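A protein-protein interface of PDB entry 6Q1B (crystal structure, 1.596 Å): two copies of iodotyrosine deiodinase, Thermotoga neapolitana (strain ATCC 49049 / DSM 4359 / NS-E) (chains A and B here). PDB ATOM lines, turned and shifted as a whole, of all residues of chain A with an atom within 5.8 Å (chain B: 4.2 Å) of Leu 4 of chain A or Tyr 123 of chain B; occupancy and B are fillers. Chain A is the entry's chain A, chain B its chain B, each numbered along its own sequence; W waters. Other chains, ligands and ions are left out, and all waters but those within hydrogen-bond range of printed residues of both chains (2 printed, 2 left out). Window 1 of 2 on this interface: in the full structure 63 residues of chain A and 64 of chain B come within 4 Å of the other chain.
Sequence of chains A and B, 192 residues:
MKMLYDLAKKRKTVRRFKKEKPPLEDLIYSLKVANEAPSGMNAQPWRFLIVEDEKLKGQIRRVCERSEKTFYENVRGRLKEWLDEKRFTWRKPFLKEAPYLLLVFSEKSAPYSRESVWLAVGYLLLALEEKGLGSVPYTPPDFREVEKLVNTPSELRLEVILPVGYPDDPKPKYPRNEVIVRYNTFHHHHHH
The backbone NH (N) of Leu 4 of chain A lies within hydrogen-bond range of the side-chain hydroxyl (OH) of Tyr 29 of chain B (3.3 Å).
N of Leu 4 of chain A sits at hydrogen-bond distance from OE2 of Glu 130 of chain B, at 2.7 Å.
OH of Tyr 29 of chain B sits at hydrogen-bond distance from N of Tyr 5 of chain A.
The side-chain hydroxyl of Tyr 5 of chain A lies within hydrogen-bond range of the side-chain carboxylate of Glu 36 of chain B (3.4 Å).
The side-chain sulfur of Met 3 of chain A sits close to the side-chain carboxylate of Glu 130 of chain B (3.6 Å).
The side-chain carboxylate of Asp 6 of chain A lies within hydrogen-bond range of the backbone NH of Met 3 of chain A (3.1 Å).
The side-chain hydroxyl of Tyr 29 of chain B is in hydrogen-bond range of the side-chain carboxylate of Glu 130 of chain B (2.4 Å).
Water W1 bridges the side-chain amino group of Lys 9 of chain A and the side-chain carboxylate of Glu 36 of chain B.
Water W2 lies within hydrogen-bond range of the guanidinium group (NH1) of Arg 11 of chain A and the backbone carbonyl oxygen (O) of Glu 36 of chain B.
Among the printed residues, merely in contact across the chains: Leu 4 of chain A with Ala 127 of chain B, Gly 122 of chain A with Tyr 123 of chain B, Tyr 123 of chain A with Gly 122 of chain B, Lys 9 of chain A with Glu 36 of chain B, Leu 126 of chain A with Leu 4 of chain B, Ala 8 of chain A with Glu 36 of chain B, Arg 11 of chain A with Tyr 123 of chain B, Tyr 123 of chain A with Leu 126 of chain B, Met 3 of chain A with Tyr 29 of chain B, Leu 126 of chain A with Tyr 123 of chain B, Leu 4 of chain A with Leu 126 of chain B, Leu 119 of chain A with Gly 122 of chain B, Arg 11 of chain A with Pro 38 of chain B, Ala 8 of chain A with Tyr 123 of chain B, Gly 122 of chain A with Leu 119 of chain B, Leu 125 of chain A with Pro 38 of chain B, Tyr 5 of chain A with Val 33 of chain B, Ala 8 of chain A with Val 33 of chain B, Val 121 of chain A with Leu 119 of chain B, Leu 119 of chain A with Leu 125 of chain B, Leu 119 of chain A with Val 121 of chain B, Leu 4 of chain A with Leu 4 of chain B, Leu 126 of chain A with Leu 126 of chain B, Leu 125 of chain A with Leu 119 of chain B, Leu 4 of chain A with Tyr 123 of chain B and Leu 4 of chain A with Val 33 of chain B.
Leu 4 of chain A touches Tyr 123 of chain B, but with the chains exchanged Tyr 123 of chain A does not touch Leu 4 of chain B (4.1 Å).
Leu 4 of chain A touches Leu 126 of chain B, and with the chains exchanged Leu 126 of chain A touches Leu 4 of chain B.
Leu 119 of chain A touches Val 121 of chain B, and with the chains exchanged Val 121 of chain A touches Leu 119 of chain B.
Leu 119 of chain A touches Gly 122 of chain B, and with the chains exchanged Gly 122 of chain A touches Leu 119 of chain B.
7 positions are printed for both chains.
Of the 31 pairs that touch across the chains among the printed residues, 14 have their exchanged pair printed and touching as well.
Of chain A, only Leu 4, Ala 8, Arg 11, Gly 122 and Leu 126 come within 4 Å of Tyr 123 of chain B.
Printed residues of chain A within 4 Å of Ala 127 of chain B: Leu 4.
Of the printed residues of chain A, Leu 119 of chain B touches Val 121 (3.8 Å), Gly 122 (3.6 Å) and Leu 125 (3.9 Å).
Printed residues of chain A within 4 Å of Leu 126 of chain B: Leu 4, Tyr 123 and Leu 126.
Of the printed residues of chain A, Pro 38 of chain B touches Arg 11 and Leu 125.
Leu 124 of chain B touches none of the printed residues of chain A.
Leu 7 of chain A touches none of the printed residues of chain B.
The nearest printed residue of chain B that does not touch Leu 4 of chain A is Leu 124 of chain B (6.0 Å).
Of the 17 printed residues of chain B, 13 touch a printed residue of chain A.
Printed residues of chain B that touch a printed residue of chain A: Leu 4, Tyr 29, Val 33, Glu 36, Pro 38, Leu 119, Val 121, Gly 122, Tyr 123, Leu 125, Leu 126, Ala 127 and Glu 130.
Printed residues of chain A that touch a printed residue of chain B: Met 3, Leu 4, Tyr 5, Ala 8, Lys 9, Arg 11, Leu 119, Val 121, Gly 122, Tyr 123, Leu 125 and Leu 126.
Hydrophobic or aromatic side chains of chain A within 4 Å of the printed part of chain B: Met 3, Leu 4, Tyr 5, Ala 8, Leu 119, Val 121, Tyr 123, Leu 125 and Leu 126.
Among the printed residues, no Asp or Glu carboxylate lies within 4 Å of a Lys or Arg side-chain nitrogen of the other chain.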
ATOM      1  N   LYS A   2     -21.554   6.060   0.824  1.00  0.00           N
ATOM      2  CA  LYS A   2     -22.809   6.044   1.566  1.00  0.00           C
ATOM      3  C   LYS A   2     -22.927   7.250   2.495  1.00  0.00           C
ATOM      4  O   LYS A   2     -23.988   7.866   2.592  1.00  0.00           O
ATOM      5  CB  LYS A   2     -22.932   4.751   2.376  1.00  0.00           C
ATOM      6  CG  LYS A   2     -23.044   3.497   1.525  1.00  0.00           C
ATOM      7  CD  LYS A   2     -23.444   2.297   2.367  1.00  0.00           C
ATOM      8  CE  LYS A   2     -23.813   1.106   1.501  1.00  0.00           C
ATOM      9  NZ  LYS A   2     -24.395   0.001   2.311  1.00  0.00           N
ATOM     10  N   MET A   3     -21.828   7.577   3.169  1.00  0.00           N
ATOM     11  CA  MET A   3     -21.793   8.663   4.147  1.00  0.00           C
ATOM     12  C   MET A   3     -20.835   9.775   3.723  1.00  0.00           C
ATOM     13  O   MET A   3     -19.942   9.584   2.896  1.00  0.00           O
ATOM     14  CB  MET A   3     -21.378   8.131   5.521  1.00  0.00           C
ATOM     15  CG  MET A   3     -22.364   7.145   6.133  1.00  0.00           C
ATOM     16  SD  MET A   3     -23.948   7.907   6.522  1.00  0.00           S
ATOM     17  CE  MET A   3     -23.480   8.960   7.892  1.00  0.00           C
ATOM     18  N   LEU A   4     -21.016  10.949   4.297  1.00  0.00           N
ATOM     19  CA  LEU A   4     -20.142  12.044   3.965  1.00  0.00           C
ATOM     20  C   LEU A   4     -18.729  11.690   4.340  1.00  0.00           C
ATOM     21  O   LEU A   4     -17.785  12.089   3.672  1.00  0.00           O
ATOM     22  CB  LEU A   4     -20.565  13.305   4.684  1.00  0.00           C
ATOM     23  CG  LEU A   4     -19.728  14.534   4.359  1.00  0.00           C
ATOM     24  CD1 LEU A   4     -19.955  14.983   2.957  1.00  0.00           C
ATOM     25  CD2 LEU A   4     -20.077  15.654   5.301  1.00  0.00           C
ATOM     26  N   TYR A   5     -18.587  10.925   5.420  1.00  0.00           N
ATOM     27  CA  TYR A   5     -17.262  10.506   5.846  1.00  0.00           C
ATOM     28  C   TYR A   5     -16.579   9.750   4.728  1.00  0.00           C
ATOM     29  O   TYR A   5     -15.390   9.901   4.510  1.00  0.00           O
ATOM     30  CB  TYR A   5     -17.325   9.635   7.106  1.00  0.00           C
ATOM     31  CG  TYR A   5     -15.969   9.112   7.492  1.00  0.00           C
ATOM     32  CD1 TYR A   5     -15.069   9.911   8.166  1.00  0.00           C
ATOM     33  CD2 TYR A   5     -15.574   7.831   7.138  1.00  0.00           C
ATOM     34  CE1 TYR A   5     -13.821   9.443   8.507  1.00  0.00           C
ATOM     35  CE2 TYR A   5     -14.327   7.356   7.473  1.00  0.00           C
ATOM     36  CZ  TYR A   5     -13.452   8.172   8.154  1.00  0.00           C
ATOM     37  OH  TYR A   5     -12.198   7.718   8.497  1.00  0.00           O
ATOM     38  N   ASP A   6     -17.322   8.917   4.019  1.00  0.00           N
ATOM     39  CA  ASP A   6     -16.705   8.094   2.995  1.00  0.00           C
ATOM     40  C   ASP A   6     -16.193   8.993   1.901  1.00  0.00           C
ATOM     41  O   ASP A   6     -15.111   8.795   1.353  1.00  0.00           O
ATOM     42  CB  ASP A   6     -17.700   7.079   2.463  1.00  0.00           C
ATOM     43  CG  ASP A   6     -18.122   6.111   3.527  1.00  0.00           C
ATOM     44  OD1 ASP A   6     -17.224   5.630   4.256  1.00  0.00           O
ATOM     45  OD2 ASP A   6     -19.336   5.861   3.660  1.00  0.00           O
ATOM     46  N   LEU A   7     -16.957  10.029   1.631  1.00  0.00           N
ATOM     47  CA  LEU A   7     -16.606  10.965   0.571  1.00  0.00           C
ATOM     48  C   LEU A   7     -15.351  11.732   0.961  1.00  0.00           C
ATOM     49  O   LEU A   7     -14.404  11.865   0.182  1.00  0.00           O
ATOM     50  CB  LEU A   7     -17.770  11.920   0.320  1.00  0.00           C
ATOM     51  CG  LEU A   7     -17.532  12.905  -0.811  1.00  0.00           C
ATOM     52  CD1 LEU A   7     -17.591  12.166  -2.147  1.00  0.00           C
ATOM     53  CD2 LEU A   7     -18.536  14.056  -0.779  1.00  0.00           C
ATOM     54  N   ALA A   8     -15.354  12.214   2.195  1.00  0.00           N
ATOM     55  CA  ALA A   8     -14.247  12.960   2.742  1.00  0.00           C
ATOM     56  C   ALA A   8     -13.039  12.076   2.837  1.00  0.00           C
ATOM     57  O   ALA A   8     -11.922  12.479   2.541  1.00  0.00           O
ATOM     58  CB  ALA A   8     -14.602  13.493   4.091  1.00  0.00           C
ATOM     59  N   LYS A   9     -13.270  10.852   3.256  1.00  0.00           N
ATOM     60  CA  LYS A   9     -12.142   9.960   3.425  1.00  0.00           C
ATOM     61  C   LYS A   9     -11.496   9.650   2.098  1.00  0.00           C
ATOM     62  O   LYS A   9     -10.265   9.588   2.006  1.00  0.00           O
ATOM     63  CB  LYS A   9     -12.568   8.665   4.103  1.00  0.00           C
ATOM     64  CG  LYS A   9     -11.436   7.655   4.168  1.00  0.00           C
ATOM     65  CD  LYS A   9     -11.616   6.681   5.309  1.00  0.00           C
ATOM     66  CE  LYS A   9     -10.395   5.786   5.470  1.00  0.00           C
ATOM     67  NZ  LYS A   9      -9.184   6.549   5.884  1.00  0.00           N
ATOM     68  N   ARG A  11     -11.613  11.422  -0.645  1.00  0.00           N
ATOM     69  CA  ARG A  11     -11.077  12.544  -1.331  1.00  0.00           C
ATOM     70  C   ARG A  11      -9.654  12.778  -0.898  1.00  0.00           C
ATOM     71  O   ARG A  11      -9.341  12.777   0.280  1.00  0.00           O
ATOM     72  CB  ARG A  11     -11.917  13.767  -1.082  1.00  0.00           C
ATOM     73  CG  ARG A  11     -11.475  14.879  -1.983  1.00  0.00           C
ATOM     74  CD  ARG A  11     -10.831  15.985  -1.249  1.00  0.00           C
ATOM     75  NE  ARG A  11     -10.144  16.814  -2.226  1.00  0.00           N
ATOM     76  CZ  ARG A  11      -8.896  17.233  -2.126  1.00  0.00           C
ATOM     77  NH1 ARG A  11      -8.183  16.989  -1.033  1.00  0.00           N
ATOM     78  NH2 ARG A  11      -8.389  17.955  -3.089  1.00  0.00           N
ATOM     79  N   LEU A 119     -13.933  27.859   4.010  1.00  0.00           N
ATOM     80  CA  LEU A 119     -15.017  26.986   4.329  1.00  0.00           C
ATOM     81  C   LEU A 119     -15.724  26.468   3.073  1.00  0.00           C
ATOM     82  O   LEU A 119     -15.956  25.288   2.891  1.00  0.00           O
ATOM     83  CB  LEU A 119     -15.980  27.735   5.226  1.00  0.00           C
ATOM     84  CG  LEU A 119     -17.022  26.933   5.963  1.00  0.00           C
ATOM     85  CD1 LEU A 119     -17.552  27.746   7.144  1.00  0.00           C
ATOM     86  CD2 LEU A 119     -18.200  26.556   5.087  1.00  0.00           C
ATOM     87  N   VAL A 121     -14.512  26.377   0.139  1.00  0.00           N
ATOM     88  CA  VAL A 121     -13.605  25.515  -0.584  1.00  0.00           C
ATOM     89  C   VAL A 121     -13.724  24.096  -0.060  1.00  0.00           C
ATOM     90  O   VAL A 121     -13.622  23.169  -0.827  1.00  0.00           O
ATOM     91  CB  VAL A 121     -12.169  26.020  -0.467  1.00  0.00           C
ATOM     92  CG1 VAL A 121     -11.178  24.974  -0.955  1.00  0.00           C
ATOM     93  CG2 VAL A 121     -12.005  27.264  -1.274  1.00  0.00           C
ATOM     94  N   GLY A 122     -13.952  23.929   1.228  1.00  0.00           N
ATOM     95  CA  GLY A 122     -14.177  22.596   1.757  1.00  0.00           C
ATOM     96  C   GLY A 122     -15.355  21.934   1.088  1.00  0.00           C
ATOM     97  O   GLY A 122     -15.339  20.784   0.667  1.00  0.00           O
ATOM     98  N   TYR A 123     -16.430  22.702   0.968  1.00  0.00           N
ATOM     99  CA  TYR A 123     -17.588  22.227   0.254  1.00  0.00           C
ATOM    100  C   TYR A 123     -17.245  21.853  -1.169  1.00  0.00           C
ATOM    101  O   TYR A 123     -17.650  20.839  -1.702  1.00  0.00           O
ATOM    102  CB  TYR A 123     -18.653  23.307   0.168  1.00  0.00           C
ATOM    103  CG  TYR A 123     -19.558  23.481   1.339  1.00  0.00           C
ATOM    104  CD1 TYR A 123     -19.091  23.426   2.640  1.00  0.00           C
ATOM    105  CD2 TYR A 123     -20.883  23.778   1.127  1.00  0.00           C
ATOM    106  CE1 TYR A 123     -19.943  23.604   3.699  1.00  0.00           C
ATOM    107  CE2 TYR A 123     -21.739  23.974   2.157  1.00  0.00           C
ATOM    108  CZ  TYR A 123     -21.268  23.911   3.445  1.00  0.00           C
ATOM    109  OH  TYR A 123     -22.139  24.108   4.503  1.00  0.00           O
ATOM    110  N   LEU A 125     -14.414  21.119  -2.565  1.00  0.00           N
ATOM    111  CA  LEU A 125     -13.617  19.937  -2.774  1.00  0.00           C
ATOM    112  C   LEU A 125     -14.438  18.694  -2.668  1.00  0.00           C
ATOM    113  O   LEU A 125     -14.207  17.753  -3.419  1.00  0.00           O
ATOM    114  CB  LEU A 125     -12.468  19.866  -1.771  1.00  0.00           C
ATOM    115  CG  LEU A 125     -11.475  21.002  -1.901  1.00  0.00           C
ATOM    116  CD1 LEU A 125     -10.365  20.741  -0.931  1.00  0.00           C
ATOM    117  CD2 LEU A 125     -10.925  21.127  -3.302  1.00  0.00           C
ATOM    118  N   LEU A 126     -15.368  18.661  -1.720  1.00  0.00           N
ATOM    119  CA  LEU A 126     -16.216  17.496  -1.588  1.00  0.00           C
ATOM    120  C   LEU A 126     -17.088  17.348  -2.813  1.00  0.00           C
ATOM    121  O   LEU A 126     -17.274  16.260  -3.325  1.00  0.00           O
ATOM    122  CB  LEU A 126     -17.053  17.574  -0.327  1.00  0.00           C
ATOM    123  CG  LEU A 126     -16.224  17.419   0.948  1.00  0.00           C
ATOM    124  CD1 LEU A 126     -17.001  17.822   2.158  1.00  0.00           C
ATOM    125  CD2 LEU A 126     -15.797  15.992   1.074  1.00  0.00           C
ATOM    126  N   LEU B   4     -24.782  15.710  -2.259  1.00  0.00           N
ATOM    127  CA  LEU B   4     -24.015  16.681  -1.508  1.00  0.00           C
ATOM    128  C   LEU B   4     -24.612  18.056  -1.654  1.00  0.00           C
ATOM    129  O   LEU B   4     -24.649  18.818  -0.695  1.00  0.00           O
ATOM    130  CB  LEU B   4     -22.573  16.697  -1.967  1.00  0.00           C
ATOM    131  CG  LEU B   4     -21.691  17.658  -1.198  1.00  0.00           C
ATOM    132  CD1 LEU B   4     -21.470  17.202   0.230  1.00  0.00           C
ATOM    133  CD2 LEU B   4     -20.390  17.756  -1.924  1.00  0.00           C
ATOM    134  N   TYR B  29     -18.256  12.072  14.888  1.00  0.00           N
ATOM    135  CA  TYR B  29     -18.351  11.753  13.487  1.00  0.00           C
ATOM    136  C   TYR B  29     -17.967  12.945  12.642  1.00  0.00           C
ATOM    137  O   TYR B  29     -17.147  12.835  11.722  1.00  0.00           O
ATOM    138  CB  TYR B  29     -19.768  11.311  13.143  1.00  0.00           C
ATOM    139  CG  TYR B  29     -20.002  11.228  11.664  1.00  0.00           C
ATOM    140  CD1 TYR B  29     -19.657  10.085  10.967  1.00  0.00           C
ATOM    141  CD2 TYR B  29     -20.543  12.299  10.959  1.00  0.00           C
ATOM    142  CE1 TYR B  29     -19.855  10.000   9.620  1.00  0.00           C
ATOM    143  CE2 TYR B  29     -20.746  12.226   9.602  1.00  0.00           C
ATOM    144  CZ  TYR B  29     -20.394  11.064   8.940  1.00  0.00           C
ATOM    145  OH  TYR B  29     -20.588  10.941   7.597  1.00  0.00           O
ATOM    146  N   VAL B  33     -14.959  13.426  10.011  1.00  0.00           N
ATOM    147  CA  VAL B  33     -15.111  13.844   8.652  1.00  0.00           C
ATOM    148  C   VAL B  33     -14.163  15.013   8.350  1.00  0.00           C
ATOM    149  O   VAL B  33     -13.424  15.003   7.375  1.00  0.00           O
ATOM    150  CB  VAL B  33     -16.535  14.271   8.364  1.00  0.00           C
ATOM    151  CG1 VAL B  33     -16.622  14.872   6.971  1.00  0.00           C
ATOM    152  CG2 VAL B  33     -17.471  13.083   8.479  1.00  0.00           C
ATOM    153  N   ALA B  34     -14.182  16.008   9.233  1.00  0.00           N
ATOM    154  CA  ALA B  34     -13.385  17.199   9.083  1.00  0.00           C
ATOM    155  C   ALA B  34     -11.916  16.826   9.023  1.00  0.00           C
ATOM    156  O   ALA B  34     -11.158  17.389   8.266  1.00  0.00           O
ATOM    157  CB  ALA B  34     -13.652  18.146  10.228  1.00  0.00           C
ATOM    158  N   GLU B  36     -10.612  14.389   7.755  1.00  0.00           N
ATOM    159  CA  GLU B  36     -10.223  13.834   6.459  1.00  0.00           C
ATOM    160  C   GLU B  36      -9.930  14.899   5.445  1.00  0.00           C
ATOM    161  O   GLU B  36      -9.481  14.600   4.332  1.00  0.00           O
ATOM    162  CB  GLU B  36     -11.322  12.941   5.913  1.00  0.00           C
ATOM    163  CG  GLU B  36     -11.474  11.709   6.715  1.00  0.00           C
ATOM    164  CD  GLU B  36     -10.262  10.837   6.618  1.00  0.00           C
ATOM    165  OE1 GLU B  36      -9.611  10.840   5.548  1.00  0.00           O
ATOM    166  OE2 GLU B  36      -9.948  10.145   7.617  1.00  0.00           O
ATOM    167  N   ALA B  37     -10.216  16.133   5.817  1.00  0.00           N
ATOM    168  CA  ALA B  37      -9.979  17.225   4.934  1.00  0.00           C
ATOM    169  C   ALA B  37      -8.502  17.369   4.658  1.00  0.00           C
ATOM    170  O   ALA B  37      -7.653  16.941   5.432  1.00  0.00           O
ATOM    171  CB  ALA B  37     -10.504  18.510   5.523  1.00  0.00           C
ATOM    172  N   PRO B  38      -8.193  17.995   3.532  1.00  0.00           N
ATOM    173  CA  PRO B  38      -6.820  18.342   3.237  1.00  0.00           C
ATOM    174  C   PRO B  38      -6.360  19.441   4.134  1.00  0.00           C
ATOM    175  O   PRO B  38      -7.157  20.118   4.790  1.00  0.00           O
ATOM    176  CB  PRO B  38      -6.886  18.830   1.799  1.00  0.00           C
ATOM    177  CG  PRO B  38      -8.251  19.363   1.661  1.00  0.00           C
ATOM    178  CD  PRO B  38      -9.103  18.444   2.467  1.00  0.00           C
ATOM    179  N   LEU B 119     -11.340  25.260   5.832  1.00  0.00           N
ATOM    180  CA  LEU B 119     -11.728  24.243   4.888  1.00  0.00           C
ATOM    181  C   LEU B 119     -12.334  23.066   5.620  1.00  0.00           C
ATOM    182  O   LEU B 119     -13.386  22.586   5.282  1.00  0.00           O
ATOM    183  CB  LEU B 119     -10.500  23.841   4.091  1.00  0.00           C
ATOM    184  CG  LEU B 119     -10.727  22.986   2.873  1.00  0.00           C
ATOM    185  CD1 LEU B 119      -9.540  23.159   1.969  1.00  0.00           C
ATOM    186  CD2 LEU B 119     -10.916  21.515   3.219  1.00  0.00           C
ATOM    187  N   ALA B 120     -11.659  22.618   6.669  1.00  0.00           N
ATOM    188  CA  ALA B 120     -12.122  21.487   7.404  1.00  0.00           C
ATOM    189  C   ALA B 120     -13.429  21.822   8.092  1.00  0.00           C
ATOM    190  O   ALA B 120     -14.289  20.958   8.241  1.00  0.00           O
ATOM    191  CB  ALA B 120     -11.050  21.048   8.400  1.00  0.00           C
ATOM    192  N   VAL B 121     -13.603  23.081   8.467  1.00  0.00           N
ATOM    193  CA  VAL B 121     -14.862  23.467   9.070  1.00  0.00           C
ATOM    194  C   VAL B 121     -15.973  23.294   8.051  1.00  0.00           C
ATOM    195  O   VAL B 121     -17.104  22.944   8.402  1.00  0.00           O
ATOM    196  CB  VAL B 121     -14.796  24.891   9.569  1.00  0.00           C
ATOM    197  CG1 VAL B 121     -16.182  25.427   9.863  1.00  0.00           C
ATOM    198  CG2 VAL B 121     -13.925  24.996  10.782  1.00  0.00           C
ATOM    199  N   GLY B 122     -15.667  23.545   6.782  1.00  0.00           N
ATOM    200  CA  GLY B 122     -16.650  23.282   5.751  1.00  0.00           C
ATOM    201  C   GLY B 122     -17.097  21.846   5.783  1.00  0.00           C
ATOM    202  O   GLY B 122     -18.251  21.520   5.768  1.00  0.00           O
ATOM    203  N   TYR B 123     -16.137  20.954   5.876  1.00  0.00           N
ATOM    204  CA  TYR B 123     -16.477  19.557   5.986  1.00  0.00           C
ATOM    205  C   TYR B 123     -17.342  19.285   7.196  1.00  0.00           C
ATOM    206  O   TYR B 123     -18.314  18.565   7.149  1.00  0.00           O
ATOM    207  CB  TYR B 123     -15.239  18.720   6.152  1.00  0.00           C
ATOM    208  CG  TYR B 123     -14.471  18.357   4.922  1.00  0.00           C
ATOM    209  CD1 TYR B 123     -14.279  19.243   3.880  1.00  0.00           C
ATOM    210  CD2 TYR B 123     -13.870  17.120   4.848  1.00  0.00           C
ATOM    211  CE1 TYR B 123     -13.532  18.900   2.797  1.00  0.00           C
ATOM    212  CE2 TYR B 123     -13.132  16.768   3.773  1.00  0.00           C
ATOM    213  CZ  TYR B 123     -12.982  17.655   2.739  1.00  0.00           C
ATOM    214  OH  TYR B 123     -12.231  17.306   1.658  1.00  0.00           O
ATOM    215  N   LEU B 124     -16.896  19.867   8.294  1.00  0.00           N
ATOM    216  CA  LEU B 124     -17.482  19.682   9.591  1.00  0.00           C
ATOM    217  C   LEU B 124     -18.927  20.071   9.538  1.00  0.00           C
ATOM    218  O   LEU B 124     -19.799  19.376  10.013  1.00  0.00           O
ATOM    219  CB  LEU B 124     -16.696  20.517  10.596  1.00  0.00           C
ATOM    220  CG  LEU B 124     -17.095  20.650  12.053  1.00  0.00           C
ATOM    221  CD1 LEU B 124     -17.672  19.405  12.579  1.00  0.00           C
ATOM    222  CD2 LEU B 124     -15.848  21.046  12.808  1.00  0.00           C
ATOM    223  N   LEU B 125     -19.180  21.220   8.962  1.00  0.00           N
ATOM    224  CA  LEU B 125     -20.549  21.685   8.952  1.00  0.00           C
ATOM    225  C   LEU B 125     -21.449  20.796   8.151  1.00  0.00           C
ATOM    226  O   LEU B 125     -22.627  20.606   8.465  1.00  0.00           O
ATOM    227  CB  LEU B 125     -20.633  23.088   8.385  1.00  0.00           C
ATOM    228  CG  LEU B 125     -19.961  24.159   9.220  1.00  0.00           C
ATOM    229  CD1 LEU B 125     -20.261  25.490   8.603  1.00  0.00           C
ATOM    230  CD2 LEU B 125     -20.436  24.122  10.650  1.00  0.00           C
ATOM    231  N   LEU B 126     -20.923  20.282   7.055  1.00  0.00           N
ATOM    232  CA  LEU B 126     -21.715  19.394   6.229  1.00  0.00           C
ATOM    233  C   LEU B 126     -21.964  18.127   6.993  1.00  0.00           C
ATOM    234  O   LEU B 126     -23.043  17.564   6.928  1.00  0.00           O
ATOM    235  CB  LEU B 126     -21.016  19.114   4.908  1.00  0.00           C
ATOM    236  CG  LEU B 126     -21.060  20.311   3.975  1.00  0.00           C
ATOM    237  CD1 LEU B 126     -20.069  20.057   2.848  1.00  0.00           C
ATOM    238  CD2 LEU B 126     -22.461  20.515   3.452  1.00  0.00           C
ATOM    239  N   ALA B 127     -20.969  17.681   7.747  1.00  0.00           N
ATOM    240  CA  ALA B 127     -21.133  16.491   8.520  1.00  0.00           C
ATOM    241  C   ALA B 127     -22.182  16.663   9.593  1.00  0.00           C
ATOM    242  O   ALA B 127     -23.005  15.791   9.788  1.00  0.00           O
ATOM    243  CB  ALA B 127     -19.799  16.097   9.128  1.00  0.00           C
ATOM    244  N   GLU B 130     -25.406  16.424   7.955  1.00  0.00           N
ATOM    245  CA  GLU B 130     -25.670  15.018   7.673  1.00  0.00           C
ATOM    246  C   GLU B 130     -26.238  14.310   8.893  1.00  0.00           C
ATOM    247  O   GLU B 130     -27.148  13.472   8.782  1.00  0.00           O
ATOM    248  CB  GLU B 130     -24.392  14.321   7.222  1.00  0.00           C
ATOM    249  CG  GLU B 130     -24.687  12.955   6.680  1.00  0.00           C
ATOM    250  CD  GLU B 130     -23.449  12.156   6.420  1.00  0.00           C
ATOM    251  OE1 GLU B 130     -22.463  12.389   7.146  1.00  0.00           O
ATOM    252  OE2 GLU B 130     -23.466  11.331   5.483  1.00  0.00           O
HETATM  253  O   HOH W   1      -7.735   8.781   5.871  1.00  0.00           O
HETATM  254  O   HOH W   2      -8.139  15.345   1.193  1.00  0.00           O
